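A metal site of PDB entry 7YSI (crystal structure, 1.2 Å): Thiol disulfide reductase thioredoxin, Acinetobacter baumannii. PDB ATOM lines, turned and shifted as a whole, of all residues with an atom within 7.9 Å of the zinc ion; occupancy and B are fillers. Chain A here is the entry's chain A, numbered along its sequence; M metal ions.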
ATOM      1  N   VAL A   8      28.716  32.413   0.518  1.00  0.00           N
ATOM      2  CA  VAL A   8      29.538  31.372  -0.092  1.00  0.00           C
ATOM      3  C   VAL A   8      28.641  30.300  -0.669  1.00  0.00           C
ATOM      4  O   VAL A   8      27.620  29.968  -0.077  1.00  0.00           O
ATOM      5  CB  VAL A   8      30.543  30.776   0.920  1.00  0.00           C
ATOM      6  CG1 VAL A   8      31.437  29.723   0.290  1.00  0.00           C
ATOM      7  CG2 VAL A   8      31.412  31.845   1.516  1.00  0.00           C
ATOM      8  N   CYS A   9      29.041  29.745  -1.808  1.00  0.00           N
ATOM      9  CA  CYS A   9      28.383  28.572  -2.367  1.00  0.00           C
ATOM     10  C   CYS A   9      29.085  27.320  -1.849  1.00  0.00           C
ATOM     11  O   CYS A   9      30.283  27.114  -2.110  1.00  0.00           O
ATOM     12  CB  CYS A   9      28.483  28.609  -3.884  1.00  0.00           C
ATOM     13  SG  CYS A   9      27.734  27.157  -4.669  1.00  0.00           S
ATOM     14  N   ALA A  10      28.350  26.459  -1.153  1.00  0.00           N
ATOM     15  CA  ALA A  10      28.941  25.236  -0.621  1.00  0.00           C
ATOM     16  C   ALA A  10      29.222  24.178  -1.700  1.00  0.00           C
ATOM     17  O   ALA A  10      29.990  23.228  -1.446  1.00  0.00           O
ATOM     18  CB  ALA A  10      27.992  24.633   0.430  1.00  0.00           C
ATOM     19  N   SER A  11      28.639  24.349  -2.883  1.00  0.00           N
ATOM     20  CA  SER A  11      28.757  23.379  -3.972  1.00  0.00           C
ATOM     21  C   SER A  11      29.999  23.618  -4.822  1.00  0.00           C
ATOM     22  O   SER A  11      30.643  22.633  -5.261  1.00  0.00           O
ATOM     23  CB  SER A  11      27.518  23.459  -4.855  1.00  0.00           C
ATOM     24  OG  SER A  11      27.451  22.328  -5.714  1.00  0.00           O
ATOM     25  N   CYS A  12      30.346  24.866  -5.125  1.00  0.00           N
ATOM     26  CA  CYS A  12      31.504  25.165  -5.943  1.00  0.00           C
ATOM     27  C   CYS A  12      32.532  26.071  -5.270  1.00  0.00           C
ATOM     28  O   CYS A  12      33.561  26.377  -5.893  1.00  0.00           O
ATOM     29  CB  CYS A  12      31.110  25.803  -7.280  1.00  0.00           C
ATOM     30  SG  CYS A  12      30.709  27.574  -7.184  1.00  0.00           S
ATOM     31  N   ASP A  13      32.274  26.542  -4.046  1.00  0.00           N
ATOM     32  CA  ASP A  13      33.149  27.386  -3.221  1.00  0.00           C
ATOM     33  C   ASP A  13      33.154  28.864  -3.594  1.00  0.00           C
ATOM     34  O   ASP A  13      33.847  29.645  -2.929  1.00  0.00           O
ATOM     35  CB  ASP A  13      34.582  26.864  -3.161  1.00  0.00           C
ATOM     36  CG  ASP A  13      34.638  25.394  -2.820  1.00  0.00           C
ATOM     37  OD1 ASP A  13      33.959  24.979  -1.868  1.00  0.00           O
ATOM     38  OD2 ASP A  13      35.298  24.619  -3.557  1.00  0.00           O
ATOM     39  N   ALA A  14      32.404  29.282  -4.611  1.00  0.00           N
ATOM     40  CA  ALA A  14      32.455  30.675  -5.027  1.00  0.00           C
ATOM     41  C   ALA A  14      31.978  31.591  -3.894  1.00  0.00           C
ATOM     42  O   ALA A  14      30.975  31.332  -3.222  1.00  0.00           O
ATOM     43  CB  ALA A  14      31.543  30.879  -6.238  1.00  0.00           C
ATOM     44  N   LYS A  15      32.691  32.686  -3.723  1.00  0.00           N
ATOM     45  CA  LYS A  15      32.329  33.727  -2.768  1.00  0.00           C
ATOM     46  C   LYS A  15      31.466  34.729  -3.534  1.00  0.00           C
ATOM     47  O   LYS A  15      31.988  35.592  -4.243  1.00  0.00           O
ATOM     48  CB  LYS A  15      33.590  34.421  -2.242  1.00  0.00           C
ATOM     49  CG  LYS A  15      34.354  33.623  -1.180  1.00  0.00           C
ATOM     50  CD  LYS A  15      34.655  32.215  -1.537  1.00  0.00           C
ATOM     51  CE  LYS A  15      35.980  32.156  -2.263  1.00  0.00           C
ATOM     52  NZ  LYS A  15      36.373  30.738  -2.500  1.00  0.00           N
ATOM     53  N   ASN A  16      30.149  34.614  -3.432  1.00  0.00           N
ATOM     54  CA  ASN A  16      29.255  35.501  -4.164  1.00  0.00           C
ATOM     55  C   ASN A  16      29.109  36.808  -3.401  1.00  0.00           C
ATOM     56  O   ASN A  16      28.883  36.816  -2.190  1.00  0.00           O
ATOM     57  CB  ASN A  16      27.869  34.854  -4.285  1.00  0.00           C
ATOM     58  CG  ASN A  16      27.832  33.771  -5.333  1.00  0.00           C
ATOM     59  OD1 ASN A  16      27.202  33.936  -6.372  1.00  0.00           O
ATOM     60  ND2 ASN A  16      28.514  32.677  -5.081  1.00  0.00           N
ATOM     61  N   SER A  28      20.725  32.496  -6.889  1.00  0.00           N
ATOM     62  CA  SER A  28      21.576  31.343  -7.144  1.00  0.00           C
ATOM     63  C   SER A  28      23.016  31.792  -7.333  1.00  0.00           C
ATOM     64  O   SER A  28      23.298  32.930  -7.660  1.00  0.00           O
ATOM     65  CB  SER A  28      21.130  30.614  -8.423  1.00  0.00           C
ATOM     66  OG  SER A  28      19.740  30.303  -8.385  1.00  0.00           O
ATOM     67  N   CYS A  29      23.924  30.849  -7.110  1.00  0.00           N
ATOM     68  CA  CYS A  29      25.351  31.104  -7.272  1.00  0.00           C
ATOM     69  C   CYS A  29      25.652  31.599  -8.672  1.00  0.00           C
ATOM     70  O   CYS A  29      25.176  31.037  -9.662  1.00  0.00           O
ATOM     71  CB  CYS A  29      26.139  29.801  -7.009  1.00  0.00           C
ATOM     72  SG  CYS A  29      27.916  29.908  -7.276  1.00  0.00           S
ATOM     73  N   GLY A  30      26.465  32.661  -8.764  1.00  0.00           N
ATOM     74  CA  GLY A  30      26.820  33.208 -10.069  1.00  0.00           C
ATOM     75  C   GLY A  30      27.719  32.315 -10.898  1.00  0.00           C
ATOM     76  O   GLY A  30      27.784  32.495 -12.127  1.00  0.00           O
ATOM     77  N   GLN A  31      28.403  31.357 -10.271  1.00  0.00           N
ATOM     78  CA  GLN A  31      29.260  30.432 -11.001  1.00  0.00           C
ATOM     79  C   GLN A  31      28.472  29.176 -11.415  1.00  0.00           C
ATOM     80  O   GLN A  31      28.366  28.879 -12.609  1.00  0.00           O
ATOM     81  CB  GLN A  31      30.474  30.032 -10.163  1.00  0.00           C
ATOM     82  CG  GLN A  31      31.436  29.057 -10.843  1.00  0.00           C
ATOM     83  CD  GLN A  31      32.606  28.597  -9.944  1.00  0.00           C
ATOM     84  OE1 GLN A  31      33.214  29.405  -9.248  1.00  0.00           O
ATOM     85  NE2 GLN A  31      32.925  27.308  -9.988  1.00  0.00           N
ATOM     86  N   CYS A  32      27.906  28.447 -10.452  1.00  0.00           N
ATOM     87  CA  CYS A  32      27.325  27.136 -10.724  1.00  0.00           C
ATOM     88  C   CYS A  32      25.811  27.101 -10.684  1.00  0.00           C
ATOM     89  O   CYS A  32      25.220  26.053 -10.995  1.00  0.00           O
ATOM     90  CB  CYS A  32      27.882  26.082  -9.766  1.00  0.00           C
ATOM     91  SG  CYS A  32      27.169  26.167  -8.100  1.00  0.00           S
ATOM     92  N   HIS A  33      25.162  28.188 -10.295  1.00  0.00           N
ATOM     93  CA  HIS A  33      23.714  28.335 -10.275  1.00  0.00           C
ATOM     94  C   HIS A  33      22.995  27.479  -9.237  1.00  0.00           C
ATOM     95  O   HIS A  33      21.760  27.374  -9.292  1.00  0.00           O
ATOM     96  CB  HIS A  33      23.061  28.112 -11.652  1.00  0.00           C
ATOM     97  CG  HIS A  33      23.589  29.004 -12.727  1.00  0.00           C
ATOM     98  ND1 HIS A  33      23.311  28.787 -14.066  1.00  0.00           N
ATOM     99  CD2 HIS A  33      24.382  30.104 -12.677  1.00  0.00           C
ATOM    100  CE1 HIS A  33      23.924  29.709 -14.780  1.00  0.00           C
ATOM    101  NE2 HIS A  33      24.568  30.526 -13.968  1.00  0.00           N
ATOM    102  N   GLN A  34      23.697  26.885  -8.274  1.00  0.00           N
ATOM    103  CA  GLN A  34      23.014  26.262  -7.155  1.00  0.00           C
ATOM    104  C   GLN A  34      22.448  27.328  -6.199  1.00  0.00           C
ATOM    105  O   GLN A  34      22.945  28.458  -6.132  1.00  0.00           O
ATOM    106  CB  GLN A  34      23.963  25.336  -6.377  1.00  0.00           C
ATOM    107  CG  GLN A  34      24.313  24.058  -7.144  1.00  0.00           C
ATOM    108  CD  GLN A  34      23.064  23.257  -7.478  1.00  0.00           C
ATOM    109  OE1 GLN A  34      22.308  22.873  -6.590  1.00  0.00           O
ATOM    110  NE2 GLN A  34      22.833  23.040  -8.761  1.00  0.00           N
ATOM    111  N   PRO A  35      21.383  27.002  -5.456  1.00  0.00           N
ATOM    112  CA  PRO A  35      20.787  28.009  -4.557  1.00  0.00           C
ATOM    113  C   PRO A  35      21.765  28.460  -3.480  1.00  0.00           C
ATOM    114  O   PRO A  35      22.400  27.651  -2.814  1.00  0.00           O
ATOM    115  CB  PRO A  35      19.565  27.278  -3.956  1.00  0.00           C
ATOM    116  CG  PRO A  35      19.250  26.140  -4.946  1.00  0.00           C
ATOM    117  CD  PRO A  35      20.631  25.722  -5.424  1.00  0.00           C
ATOM    118  N   LEU A  36      21.859  29.765  -3.269  1.00  0.00           N
ATOM    119  CA  LEU A  36      22.750  30.282  -2.223  1.00  0.00           C
ATOM    120  C   LEU A  36      22.097  30.324  -0.865  1.00  0.00           C
ATOM    121  O   LEU A  36      22.771  30.179   0.160  1.00  0.00           O
ATOM    122  CB  LEU A  36      23.218  31.705  -2.564  1.00  0.00           C
ATOM    123  CG  LEU A  36      24.197  31.823  -3.715  1.00  0.00           C
ATOM    124  CD1 LEU A  36      24.367  33.287  -4.060  1.00  0.00           C
ATOM    125  CD2 LEU A  36      25.516  31.201  -3.341  1.00  0.00           C
HETATM  126 ZN    ZN M   1      28.439  27.674  -6.869  1.00  0.00          ZN
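The nearest printed residue that does not touch the zinc ion is Ala 14 (4.5 Å).
SG of Cys 12 binds the zinc ion, at 2.3 Å.
The side-chain sulfur (SG) of Cys 32 is bound to the zinc ion (2.3 Å).
The zinc ion is bound by SG of Cys 29.
The side-chain sulfur (SG) of Cys 9 is bound to the zinc ion, 2.4 Å away.
The zinc ion has four donor atoms within binding distance.
The side-chain sulfur (SG) of Cys 12 sits close to the backbone NH (N) of Ala 14.
The side-chain amide nitrogen (NE2) of Gln 31 sits close to the side-chain sulfur (SG) of Cys 12, at 3.6 Å.
The side-chain sulfur of Cys 32 lies close to the backbone NH of Gln 34.
The side-chain sulfur of Cys 29 sits close to the backbone NH of Gln 31, 3.4 Å away.
O of Gln 34 lies within hydrogen-bond range of N of Cys 29, 2.8 Å away.
The side-chain sulfur (SG) of Cys 29 lies close to the side-chain amide nitrogen (ND2) of Asn 16, at 3.6 Å.
N of Cys 9 lies within hydrogen-bond range of O of Ala 14 (2.9 Å).
SG of Cys 9 lies close to N of Ser 11.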
